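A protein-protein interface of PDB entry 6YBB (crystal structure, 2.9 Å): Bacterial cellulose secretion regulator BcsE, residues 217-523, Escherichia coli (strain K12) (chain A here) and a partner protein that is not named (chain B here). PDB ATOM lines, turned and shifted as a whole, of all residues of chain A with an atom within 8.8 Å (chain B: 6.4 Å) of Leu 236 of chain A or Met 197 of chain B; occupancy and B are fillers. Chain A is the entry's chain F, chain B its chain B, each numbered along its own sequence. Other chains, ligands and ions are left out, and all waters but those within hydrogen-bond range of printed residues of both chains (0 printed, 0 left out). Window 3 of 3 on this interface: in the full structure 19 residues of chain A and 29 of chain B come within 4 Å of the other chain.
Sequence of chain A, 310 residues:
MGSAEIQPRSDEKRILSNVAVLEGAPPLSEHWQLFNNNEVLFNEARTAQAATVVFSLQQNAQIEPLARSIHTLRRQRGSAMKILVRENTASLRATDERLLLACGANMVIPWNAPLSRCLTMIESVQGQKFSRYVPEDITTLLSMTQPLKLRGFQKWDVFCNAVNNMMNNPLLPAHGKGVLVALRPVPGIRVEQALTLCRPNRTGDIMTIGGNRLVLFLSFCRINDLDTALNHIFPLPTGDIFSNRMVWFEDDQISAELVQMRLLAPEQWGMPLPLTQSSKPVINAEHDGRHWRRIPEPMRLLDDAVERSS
OG1 of Thr 230 of chain B sits at hydrogen-bond distance from NH1 of Arg 199 of chain A, at 2.7 Å.
The backbone NH (N) of Arg 199 of chain A lies within hydrogen-bond range of the backbone carbonyl oxygen (O) of Ile 233 of chain A (2.9 Å). N of Leu 231 of chain B lies close to SD of Met 197 of chain B, 3.6 Å away.
Printed residues of chain B within 4 Å of Arg 199 of chain A: Thr 230 (2.7 Å). Leu 230 of chain A touches none of the printed residues of chain B. Printed residues of chain B within 4 Å of Leu 236 of chain A: Met 197 (3.8 Å) and Thr 230 (3.9 Å). Of chain A, only Leu 236 comes within 4 Å of Met 197 of chain B. Printed residues of chain A within 4 Å of Thr 230 of chain B: Arg 199 (2.7 Å), Pro 235 (3.7 Å) and Leu 236 (3.9 Å). Of the printed residues of chain A, Leu 237 of chain B touches Ile 189 (3.8 Å). The nearest residue of chain A that does not touch Met 197 of chain B is Pro 235 of chain A (6.7 Å). The nearest printed residue of chain A that does not touch Asn 233 of chain B is Leu 236 of chain A (4.8 Å).
Of the 18 printed residues of chain B, 4 touch a printed residue of chain A. Hydrophobic or aromatic side chains of chain B within 4 Å of the printed part of chain A: Met 197 and Leu 237. Among the printed residues, 7 pairs touch across the chains.
Among the printed residues, pairs that only touch across the chains: Leu 197 of chain A with Asn 233 of chain B, Pro 235 of chain A with Thr 230 of chain B, Leu 236 of chain A with Met 197 of chain B, Ile 189 of chain A with Leu 237 of chain B, Ile 189 of chain A with Asn 233 of chain B and Leu 236 of chain A with Thr 230 of chain B.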
ATOM      1  N   ILE A 189     -18.334  16.716  13.447  1.00  0.00           N
ATOM      2  CA  ILE A 189     -18.806  18.015  13.908  1.00  0.00           C
ATOM      3  C   ILE A 189     -17.859  19.092  13.396  1.00  0.00           C
ATOM      4  O   ILE A 189     -16.667  18.850  13.181  1.00  0.00           O
ATOM      5  CB  ILE A 189     -18.925  18.062  15.453  1.00  0.00           C
ATOM      6  CG1 ILE A 189     -19.662  19.324  15.916  1.00  0.00           C
ATOM      7  CG2 ILE A 189     -17.553  17.968  16.108  1.00  0.00           C
ATOM      8  CD1 ILE A 189     -20.025  19.314  17.388  1.00  0.00           C
ATOM      9  N   LEU A 197     -20.945  23.890  22.344  1.00  0.00           N
ATOM     10  CA  LEU A 197     -20.852  22.940  23.447  1.00  0.00           C
ATOM     11  C   LEU A 197     -19.964  23.446  24.578  1.00  0.00           C
ATOM     12  O   LEU A 197     -20.182  23.082  25.738  1.00  0.00           O
ATOM     13  CB  LEU A 197     -20.333  21.593  22.947  1.00  0.00           C
ATOM     14  CG  LEU A 197     -21.396  20.657  22.377  1.00  0.00           C
ATOM     15  CD1 LEU A 197     -20.760  19.369  21.898  1.00  0.00           C
ATOM     16  CD2 LEU A 197     -22.469  20.372  23.420  1.00  0.00           C
ATOM     17  N   CYS A 198     -18.971  24.275  24.270  1.00  0.00           N
ATOM     18  CA  CYS A 198     -18.025  24.761  25.272  1.00  0.00           C
ATOM     19  C   CYS A 198     -18.654  25.938  26.012  1.00  0.00           C
ATOM     20  O   CYS A 198     -18.680  27.063  25.508  1.00  0.00           O
ATOM     21  CB  CYS A 198     -16.712  25.155  24.607  1.00  0.00           C
ATOM     22  SG  CYS A 198     -15.349  25.435  25.746  1.00  0.00           S
ATOM     23  N   ARG A 199     -19.160  25.684  27.218  1.00  0.00           N
ATOM     24  CA  ARG A 199     -19.879  26.692  28.000  1.00  0.00           C
ATOM     25  C   ARG A 199     -19.136  26.972  29.298  1.00  0.00           C
ATOM     26  O   ARG A 199     -19.333  26.255  30.296  1.00  0.00           O
ATOM     27  CB  ARG A 199     -21.308  26.235  28.287  1.00  0.00           C
ATOM     28  CG  ARG A 199     -21.943  25.476  27.133  1.00  0.00           C
ATOM     29  CD  ARG A 199     -23.457  25.544  27.165  1.00  0.00           C
ATOM     30  NE  ARG A 199     -24.048  24.705  26.127  1.00  0.00           N
ATOM     31  CZ  ARG A 199     -24.648  23.541  26.356  1.00  0.00           C
ATOM     32  NH1 ARG A 199     -25.153  22.844  25.347  1.00  0.00           N
ATOM     33  NH2 ARG A 199     -24.756  23.082  27.597  1.00  0.00           N
ATOM     34  N   ASP A 227      -8.655  17.962  33.377  1.00  0.00           N
ATOM     35  CA  ASP A 227      -9.762  17.134  32.910  1.00  0.00           C
ATOM     36  C   ASP A 227     -11.028  17.397  33.715  1.00  0.00           C
ATOM     37  O   ASP A 227     -12.132  17.420  33.158  1.00  0.00           O
ATOM     38  CB  ASP A 227      -9.377  15.656  32.973  1.00  0.00           C
ATOM     39  CG  ASP A 227      -8.471  15.237  31.826  1.00  0.00           C
ATOM     40  OD1 ASP A 227      -8.295  16.030  30.875  1.00  0.00           O
ATOM     41  OD2 ASP A 227      -7.934  14.111  31.876  1.00  0.00           O
ATOM     42  N   LEU A 230     -12.563  20.514  32.440  1.00  0.00           N
ATOM     43  CA  LEU A 230     -13.260  20.340  31.169  1.00  0.00           C
ATOM     44  C   LEU A 230     -14.643  19.737  31.377  1.00  0.00           C
ATOM     45  O   LEU A 230     -15.589  20.087  30.662  1.00  0.00           O
ATOM     46  CB  LEU A 230     -12.427  19.471  30.227  1.00  0.00           C
ATOM     47  CG  LEU A 230     -11.067  20.036  29.810  1.00  0.00           C
ATOM     48  CD1 LEU A 230     -10.319  19.036  28.944  1.00  0.00           C
ATOM     49  CD2 LEU A 230     -11.228  21.365  29.085  1.00  0.00           C
ATOM     50  N   ASN A 231     -14.784  18.831  32.349  1.00  0.00           N
ATOM     51  CA  ASN A 231     -16.102  18.288  32.659  1.00  0.00           C
ATOM     52  C   ASN A 231     -17.071  19.363  33.127  1.00  0.00           C
ATOM     53  O   ASN A 231     -18.287  19.181  33.004  1.00  0.00           O
ATOM     54  CB  ASN A 231     -15.991  17.198  33.724  1.00  0.00           C
ATOM     55  CG  ASN A 231     -15.247  15.979  33.232  1.00  0.00           C
ATOM     56  OD1 ASN A 231     -14.554  16.029  32.214  1.00  0.00           O
ATOM     57  ND2 ASN A 231     -15.386  14.870  33.951  1.00  0.00           N
ATOM     58  N   HIS A 232     -16.559  20.476  33.663  1.00  0.00           N
ATOM     59  CA  HIS A 232     -17.404  21.590  34.072  1.00  0.00           C
ATOM     60  C   HIS A 232     -17.789  22.493  32.909  1.00  0.00           C
ATOM     61  O   HIS A 232     -18.764  23.245  33.021  1.00  0.00           O
ATOM     62  CB  HIS A 232     -16.696  22.420  35.145  1.00  0.00           C
ATOM     63  CG  HIS A 232     -16.525  21.702  36.448  1.00  0.00           C
ATOM     64  ND1 HIS A 232     -15.718  22.178  37.459  1.00  0.00           N
ATOM     65  CD2 HIS A 232     -17.059  20.546  36.906  1.00  0.00           C
ATOM     66  CE1 HIS A 232     -15.761  21.344  38.482  1.00  0.00           C
ATOM     67  NE2 HIS A 232     -16.568  20.345  38.173  1.00  0.00           N
ATOM     68  N   ILE A 233     -17.056  22.430  31.801  1.00  0.00           N
ATOM     69  CA  ILE A 233     -17.290  23.310  30.672  1.00  0.00           C
ATOM     70  C   ILE A 233     -17.958  22.596  29.501  1.00  0.00           C
ATOM     71  O   ILE A 233     -18.644  23.248  28.704  1.00  0.00           O
ATOM     72  CB  ILE A 233     -15.965  23.966  30.233  1.00  0.00           C
ATOM     73  CG1 ILE A 233     -15.243  24.537  31.451  1.00  0.00           C
ATOM     74  CG2 ILE A 233     -16.206  25.075  29.229  1.00  0.00           C
ATOM     75  CD1 ILE A 233     -13.879  25.090  31.147  1.00  0.00           C
ATOM     76  N   PHE A 234     -17.798  21.278  29.380  1.00  0.00           N
ATOM     77  CA  PHE A 234     -18.412  20.517  28.303  1.00  0.00           C
ATOM     78  C   PHE A 234     -19.488  19.594  28.849  1.00  0.00           C
ATOM     79  O   PHE A 234     -19.236  18.860  29.813  1.00  0.00           O
ATOM     80  CB  PHE A 234     -17.360  19.693  27.553  1.00  0.00           C
ATOM     81  CG  PHE A 234     -16.414  20.520  26.736  1.00  0.00           C
ATOM     82  CD1 PHE A 234     -16.773  20.958  25.474  1.00  0.00           C
ATOM     83  CD2 PHE A 234     -15.165  20.858  27.227  1.00  0.00           C
ATOM     84  CE1 PHE A 234     -15.904  21.719  24.717  1.00  0.00           C
ATOM     85  CE2 PHE A 234     -14.291  21.616  26.475  1.00  0.00           C
ATOM     86  CZ  PHE A 234     -14.662  22.048  25.218  1.00  0.00           C
ATOM     87  N   PRO A 235     -20.693  19.605  28.270  1.00  0.00           N
ATOM     88  CA  PRO A 235     -21.723  18.656  28.730  1.00  0.00           C
ATOM     89  C   PRO A 235     -21.406  17.218  28.367  1.00  0.00           C
ATOM     90  O   PRO A 235     -21.669  16.308  29.162  1.00  0.00           O
ATOM     91  CB  PRO A 235     -22.997  19.147  28.028  1.00  0.00           C
ATOM     92  CG  PRO A 235     -22.691  20.545  27.583  1.00  0.00           C
ATOM     93  CD  PRO A 235     -21.226  20.577  27.306  1.00  0.00           C
ATOM     94  N   LEU A 236     -20.856  16.987  27.189  1.00  0.00           N
ATOM     95  CA  LEU A 236     -20.466  15.672  26.712  1.00  0.00           C
ATOM     96  C   LEU A 236     -18.973  15.457  26.912  1.00  0.00           C
ATOM     97  O   LEU A 236     -18.204  16.419  27.004  1.00  0.00           O
ATOM     98  CB  LEU A 236     -20.827  15.525  25.229  1.00  0.00           C
ATOM     99  CG  LEU A 236     -22.319  15.628  24.908  1.00  0.00           C
ATOM    100  CD1 LEU A 236     -22.546  15.709  23.412  1.00  0.00           C
ATOM    101  CD2 LEU A 236     -23.064  14.445  25.493  1.00  0.00           C
ATOM    102  N   PRO A 237     -18.526  14.202  26.999  1.00  0.00           N
ATOM    103  CA  PRO A 237     -17.093  13.943  27.193  1.00  0.00           C
ATOM    104  C   PRO A 237     -16.261  14.552  26.075  1.00  0.00           C
ATOM    105  O   PRO A 237     -16.646  14.525  24.905  1.00  0.00           O
ATOM    106  CB  PRO A 237     -17.006  12.412  27.187  1.00  0.00           C
ATOM    107  CG  PRO A 237     -18.366  11.955  27.576  1.00  0.00           C
ATOM    108  CD  PRO A 237     -19.313  12.957  26.987  1.00  0.00           C
ATOM    109  N   THR A 238     -15.107  15.111  26.450  1.00  0.00           N
ATOM    110  CA  THR A 238     -14.265  15.784  25.466  1.00  0.00           C
ATOM    111  C   THR A 238     -13.679  14.804  24.458  1.00  0.00           C
ATOM    112  O   THR A 238     -13.411  15.186  23.313  1.00  0.00           O
ATOM    113  CB  THR A 238     -13.143  16.554  26.163  1.00  0.00           C
ATOM    114  OG1 THR A 238     -12.397  15.662  26.998  1.00  0.00           O
ATOM    115  CG2 THR A 238     -13.720  17.674  27.010  1.00  0.00           C
ATOM    116  N   GLY A 239     -13.474  13.548  24.859  1.00  0.00           N
ATOM    117  CA  GLY A 239     -12.976  12.556  23.923  1.00  0.00           C
ATOM    118  C   GLY A 239     -13.944  12.275  22.792  1.00  0.00           C
ATOM    119  O   GLY A 239     -13.527  11.911  21.689  1.00  0.00           O
ATOM    120  N   ASP A 240     -15.244  12.446  23.043  1.00  0.00           N
ATOM    121  CA  ASP A 240     -16.248  12.230  22.007  1.00  0.00           C
ATOM    122  C   ASP A 240     -16.373  13.425  21.071  1.00  0.00           C
ATOM    123  O   ASP A 240     -16.744  13.256  19.905  1.00  0.00           O
ATOM    124  CB  ASP A 240     -17.603  11.930  22.644  1.00  0.00           C
ATOM    125  CG  ASP A 240     -17.552  10.746  23.583  1.00  0.00           C
ATOM    126  OD1 ASP A 240     -16.482  10.106  23.665  1.00  0.00           O
ATOM    127  OD2 ASP A 240     -18.577  10.458  24.240  1.00  0.00           O
ATOM    128  N   ILE A 241     -16.076  14.629  21.557  1.00  0.00           N
ATOM    129  CA  ILE A 241     -16.200  15.816  20.719  1.00  0.00           C
ATOM    130  C   ILE A 241     -14.934  16.036  19.907  1.00  0.00           C
ATOM    131  O   ILE A 241     -14.996  16.418  18.733  1.00  0.00           O
ATOM    132  CB  ILE A 241     -16.530  17.043  21.586  1.00  0.00           C
ATOM    133  CG1 ILE A 241     -17.779  16.780  22.435  1.00  0.00           C
ATOM    134  CG2 ILE A 241     -16.701  18.280  20.711  1.00  0.00           C
ATOM    135  CD1 ILE A 241     -17.987  17.783  23.560  1.00  0.00           C
ATOM    136  N   PHE A 242     -13.772  15.802  20.509  1.00  0.00           N
ATOM    137  CA  PHE A 242     -12.497  16.130  19.896  1.00  0.00           C
ATOM    138  C   PHE A 242     -11.640  14.882  19.744  1.00  0.00           C
ATOM    139  O   PHE A 242     -11.704  13.955  20.558  1.00  0.00           O
ATOM    140  CB  PHE A 242     -11.744  17.179  20.720  1.00  0.00           C
ATOM    141  CG  PHE A 242     -12.572  18.382  21.062  1.00  0.00           C
ATOM    142  CD1 PHE A 242     -12.803  19.372  20.120  1.00  0.00           C
ATOM    143  CD2 PHE A 242     -13.128  18.521  22.324  1.00  0.00           C
ATOM    144  CE1 PHE A 242     -13.569  20.479  20.434  1.00  0.00           C
ATOM    145  CE2 PHE A 242     -13.895  19.625  22.643  1.00  0.00           C
ATOM    146  CZ  PHE A 242     -14.115  20.606  21.698  1.00  0.00           C
ATOM    147  N   ILE B 168     -33.490   6.413  24.239  1.00  0.00           N
ATOM    148  CA  ILE B 168     -34.511   6.932  25.139  1.00  0.00           C
ATOM    149  C   ILE B 168     -34.072   8.294  25.661  1.00  0.00           C
ATOM    150  O   ILE B 168     -32.939   8.456  26.128  1.00  0.00           O
ATOM    151  CB  ILE B 168     -34.767   5.948  26.290  1.00  0.00           C
ATOM    152  CG1 ILE B 168     -35.280   4.618  25.730  1.00  0.00           C
ATOM    153  CG2 ILE B 168     -35.742   6.535  27.296  1.00  0.00           C
ATOM    154  CD1 ILE B 168     -35.350   3.509  26.748  1.00  0.00           C
ATOM    155  N   LEU B 169     -34.968   9.276  25.573  1.00  0.00           N
ATOM    156  CA  LEU B 169     -34.723  10.627  26.061  1.00  0.00           C
ATOM    157  C   LEU B 169     -35.666  10.923  27.218  1.00  0.00           C
ATOM    158  O   LEU B 169     -36.869  10.659  27.128  1.00  0.00           O
ATOM    159  CB  LEU B 169     -34.912  11.662  24.949  1.00  0.00           C
ATOM    160  CG  LEU B 169     -34.837  13.127  25.381  1.00  0.00           C
ATOM    161  CD1 LEU B 169     -33.459  13.446  25.931  1.00  0.00           C
ATOM    162  CD2 LEU B 169     -35.179  14.041  24.221  1.00  0.00           C
ATOM    163  N   ILE B 170     -35.119  11.482  28.296  1.00  0.00           N
ATOM    164  CA  ILE B 170     -35.871  11.786  29.507  1.00  0.00           C
ATOM    165  C   ILE B 170     -36.265  13.256  29.487  1.00  0.00           C
ATOM    166  O   ILE B 170     -35.424  14.131  29.246  1.00  0.00           O
ATOM    167  CB  ILE B 170     -35.048  11.449  30.764  1.00  0.00           C
ATOM    168  CG1 ILE B 170     -35.031   9.937  31.006  1.00  0.00           C
ATOM    169  CG2 ILE B 170     -35.582  12.184  31.979  1.00  0.00           C
ATOM    170  CD1 ILE B 170     -34.182   9.520  32.187  1.00  0.00           C
ATOM    171  N   LEU B 194     -30.401   4.329  27.219  1.00  0.00           N
ATOM    172  CA  LEU B 194     -30.566   5.679  27.736  1.00  0.00           C
ATOM    173  C   LEU B 194     -29.537   6.624  27.125  1.00  0.00           C
ATOM    174  O   LEU B 194     -28.440   6.220  26.733  1.00  0.00           O
ATOM    175  CB  LEU B 194     -30.445   5.684  29.258  1.00  0.00           C
ATOM    176  CG  LEU B 194     -31.525   6.451  30.024  1.00  0.00           C
ATOM    177  CD1 LEU B 194     -32.909   5.976  29.616  1.00  0.00           C
ATOM    178  CD2 LEU B 194     -31.330   6.295  31.522  1.00  0.00           C
ATOM    179  N   LEU B 195     -29.908   7.895  27.046  1.00  0.00           N
ATOM    180  CA  LEU B 195     -29.029   8.924  26.520  1.00  0.00           C
ATOM    181  C   LEU B 195     -28.114   9.459  27.618  1.00  0.00           C
ATOM    182  O   LEU B 195     -28.375   9.264  28.807  1.00  0.00           O
ATOM    183  CB  LEU B 195     -29.861  10.052  25.915  1.00  0.00           C
ATOM    184  CG  LEU B 195     -30.450   9.755  24.537  1.00  0.00           C
ATOM    185  CD1 LEU B 195     -31.092  10.999  23.944  1.00  0.00           C
ATOM    186  CD2 LEU B 195     -29.376   9.205  23.609  1.00  0.00           C
ATOM    187  N   PRO B 196     -27.016  10.124  27.248  1.00  0.00           N
ATOM    188  CA  PRO B 196     -26.140  10.736  28.253  1.00  0.00           C
ATOM    189  C   PRO B 196     -26.618  12.085  28.765  1.00  0.00           C
ATOM    190  O   PRO B 196     -25.866  12.757  29.476  1.00  0.00           O
ATOM    191  CB  PRO B 196     -24.819  10.887  27.489  1.00  0.00           C
ATOM    192  CG  PRO B 196     -25.254  11.150  26.097  1.00  0.00           C
ATOM    193  CD  PRO B 196     -26.478  10.293  25.885  1.00  0.00           C
ATOM    194  N   MET B 197     -27.835  12.492  28.419  1.00  0.00           N
ATOM    195  CA  MET B 197     -28.370  13.783  28.818  1.00  0.00           C
ATOM    196  C   MET B 197     -29.869  13.644  29.038  1.00  0.00           C
ATOM    197  O   MET B 197     -30.493  12.664  28.618  1.00  0.00           O
ATOM    198  CB  MET B 197     -28.100  14.847  27.757  1.00  0.00           C
ATOM    199  CG  MET B 197     -28.994  14.671  26.548  1.00  0.00           C
ATOM    200  SD  MET B 197     -28.256  15.224  25.016  1.00  0.00           S
ATOM    201  CE  MET B 197     -26.774  14.223  24.977  1.00  0.00           C
ATOM    202  N   LEU B 198     -30.446  14.649  29.688  1.00  0.00           N
ATOM    203  CA  LEU B 198     -31.881  14.677  29.912  1.00  0.00           C
ATOM    204  C   LEU B 198     -32.336  16.124  29.997  1.00  0.00           C
ATOM    205  O   LEU B 198     -31.537  17.035  30.230  1.00  0.00           O
ATOM    206  CB  LEU B 198     -32.274  13.898  31.176  1.00  0.00           C
ATOM    207  CG  LEU B 198     -31.434  14.071  32.445  1.00  0.00           C
ATOM    208  CD1 LEU B 198     -31.773  15.360  33.184  1.00  0.00           C
ATOM    209  CD2 LEU B 198     -31.600  12.866  33.361  1.00  0.00           C
ATOM    210  N   ILE B 199     -33.632  16.321  29.807  1.00  0.00           N
ATOM    211  CA  ILE B 199     -34.233  17.646  29.756  1.00  0.00           C
ATOM    212  C   ILE B 199     -35.006  17.848  31.052  1.00  0.00           C
ATOM    213  O   ILE B 199     -36.029  17.192  31.287  1.00  0.00           O
ATOM    214  CB  ILE B 199     -35.134  17.808  28.526  1.00  0.00           C
ATOM    215  CG1 ILE B 199     -34.380  17.370  27.268  1.00  0.00           C
ATOM    216  CG2 ILE B 199     -35.595  19.244  28.387  1.00  0.00           C
ATOM    217  CD1 ILE B 199     -35.244  17.312  26.038  1.00  0.00           C
ATOM    218  N   GLU B 227     -29.922  22.135  27.199  1.00  0.00           N
ATOM    219  CA  GLU B 227     -29.912  20.677  27.211  1.00  0.00           C
ATOM    220  C   GLU B 227     -30.325  20.115  25.857  1.00  0.00           C
ATOM    221  O   GLU B 227     -29.781  19.099  25.407  1.00  0.00           O
ATOM    222  CB  GLU B 227     -30.826  20.157  28.322  1.00  0.00           C
ATOM    223  CG  GLU B 227     -30.245  20.329  29.719  1.00  0.00           C
ATOM    224  CD  GLU B 227     -31.281  20.181  30.824  1.00  0.00           C
ATOM    225  OE1 GLU B 227     -32.493  20.244  30.528  1.00  0.00           O
ATOM    226  OE2 GLU B 227     -30.876  20.007  31.994  1.00  0.00           O
ATOM    227  N   ILE B 228     -31.281  20.764  25.190  1.00  0.00           N
ATOM    228  CA  ILE B 228     -31.674  20.328  23.854  1.00  0.00           C
ATOM    229  C   ILE B 228     -30.606  20.705  22.835  1.00  0.00           C
ATOM    230  O   ILE B 228     -30.371  19.965  21.871  1.00  0.00           O
ATOM    231  CB  ILE B 228     -33.055  20.907  23.497  1.00  0.00           C
ATOM    232  CG1 ILE B 228     -34.115  20.337  24.445  1.00  0.00           C
ATOM    233  CG2 ILE B 228     -33.417  20.590  22.058  1.00  0.00           C
ATOM    234  CD1 ILE B 228     -35.461  21.015  24.363  1.00  0.00           C
ATOM    235  N   THR B 230     -27.502  20.579  23.530  1.00  0.00           N
ATOM    236  CA  THR B 230     -26.593  19.451  23.695  1.00  0.00           C
ATOM    237  C   THR B 230     -27.107  18.221  22.958  1.00  0.00           C
ATOM    238  O   THR B 230     -26.311  17.413  22.465  1.00  0.00           O
ATOM    239  CB  THR B 230     -26.397  19.146  25.182  1.00  0.00           C
ATOM    240  OG1 THR B 230     -25.942  20.325  25.858  1.00  0.00           O
ATOM    241  CG2 THR B 230     -25.371  18.039  25.378  1.00  0.00           C
ATOM    242  N   LEU B 231     -28.430  18.072  22.859  1.00  0.00           N
ATOM    243  CA  LEU B 231     -28.994  16.948  22.118  1.00  0.00           C
ATOM    244  C   LEU B 231     -28.699  17.069  20.630  1.00  0.00           C
ATOM    245  O   LEU B 231     -28.364  16.075  19.974  1.00  0.00           O
ATOM    246  CB  LEU B 231     -30.500  16.863  22.375  1.00  0.00           C
ATOM    247  CG  LEU B 231     -31.318  15.760  21.701  1.00  0.00           C
ATOM    248  CD1 LEU B 231     -30.819  14.380  22.096  1.00  0.00           C
ATOM    249  CD2 LEU B 231     -32.787  15.924  22.055  1.00  0.00           C
ATOM    250  N   ALA B 232     -28.804  18.284  20.086  1.00  0.00           N
ATOM    251  CA  ALA B 232     -28.488  18.508  18.679  1.00  0.00           C
ATOM    252  C   ALA B 232     -27.039  18.149  18.374  1.00  0.00           C
ATOM    253  O   ALA B 232     -26.752  17.481  17.375  1.00  0.00           O
ATOM    254  CB  ALA B 232     -28.773  19.962  18.306  1.00  0.00           C
ATOM    255  N   ASN B 233     -26.108  18.589  19.224  1.00  0.00           N
ATOM    256  CA  ASN B 233     -24.704  18.258  19.006  1.00  0.00           C
ATOM    257  C   ASN B 233     -24.469  16.760  19.130  1.00  0.00           C
ATOM    258  O   ASN B 233     -23.635  16.193  18.415  1.00  0.00           O
ATOM    259  CB  ASN B 233     -23.818  19.025  19.988  1.00  0.00           C
ATOM    260  CG  ASN B 233     -23.802  20.519  19.719  1.00  0.00           C
ATOM    261  OD1 ASN B 233     -23.138  20.988  18.794  1.00  0.00           O
ATOM    262  ND2 ASN B 233     -24.529  21.275  20.534  1.00  0.00           N
ATOM    263  N   TRP B 234     -25.199  16.097  20.034  1.00  0.00           N
ATOM    264  CA  TRP B 234     -25.102  14.645  20.144  1.00  0.00           C
ATOM    265  C   TRP B 234     -25.636  13.967  18.888  1.00  0.00           C
ATOM    266  O   TRP B 234     -25.078  12.962  18.432  1.00  0.00           O
ATOM    267  CB  TRP B 234     -25.852  14.154  21.384  1.00  0.00           C
ATOM    268  CG  TRP B 234     -25.666  12.683  21.654  1.00  0.00           C
ATOM    269  CD1 TRP B 234     -24.700  12.108  22.431  1.00  0.00           C
ATOM    270  CD2 TRP B 234     -26.463  11.606  21.143  1.00  0.00           C
ATOM    271  NE1 TRP B 234     -24.848  10.741  22.436  1.00  0.00           N
ATOM    272  CE2 TRP B 234     -25.921  10.407  21.652  1.00  0.00           C
ATOM    273  CE3 TRP B 234     -27.580  11.537  20.304  1.00  0.00           C
ATOM    274  CZ2 TRP B 234     -26.459   9.157  21.351  1.00  0.00           C
ATOM    275  CZ3 TRP B 234     -28.112  10.293  20.004  1.00  0.00           C
ATOM    276  CH2 TRP B 234     -27.551   9.122  20.528  1.00  0.00           C
ATOM    277  N   LEU B 237     -23.084  13.998  16.197  1.00  0.00           N
ATOM    278  CA  LEU B 237     -21.974  13.086  16.416  1.00  0.00           C
ATOM    279  C   LEU B 237     -22.376  11.624  16.298  1.00  0.00           C
ATOM    280  O   LEU B 237     -21.519  10.783  16.003  1.00  0.00           O
ATOM    281  CB  LEU B 237     -21.356  13.344  17.790  1.00  0.00           C
ATOM    282  CG  LEU B 237     -20.668  14.685  18.041  1.00  0.00           C
ATOM    283  CD1 LEU B 237     -20.403  14.852  19.522  1.00  0.00           C
ATOM    284  CD2 LEU B 237     -19.370  14.751  17.271  1.00  0.00           C
ATOM    285  N   ASN B 238     -23.655  11.300  16.494  1.00  0.00           N
ATOM    286  CA  ASN B 238     -24.088   9.910  16.552  1.00  0.00           C
ATOM    287  C   ASN B 238     -25.190   9.537  15.573  1.00  0.00           C
ATOM    288  O   ASN B 238     -25.328   8.344  15.275  1.00  0.00           O
ATOM    289  CB  ASN B 238     -24.566   9.559  17.969  1.00  0.00           C
ATOM    290  CG  ASN B 238     -23.466   9.683  18.998  1.00  0.00           C
ATOM    291  OD1 ASN B 238     -22.801   8.703  19.331  1.00  0.00           O
ATOM    292  ND2 ASN B 238     -23.259  10.895  19.502  1.00  0.00           N
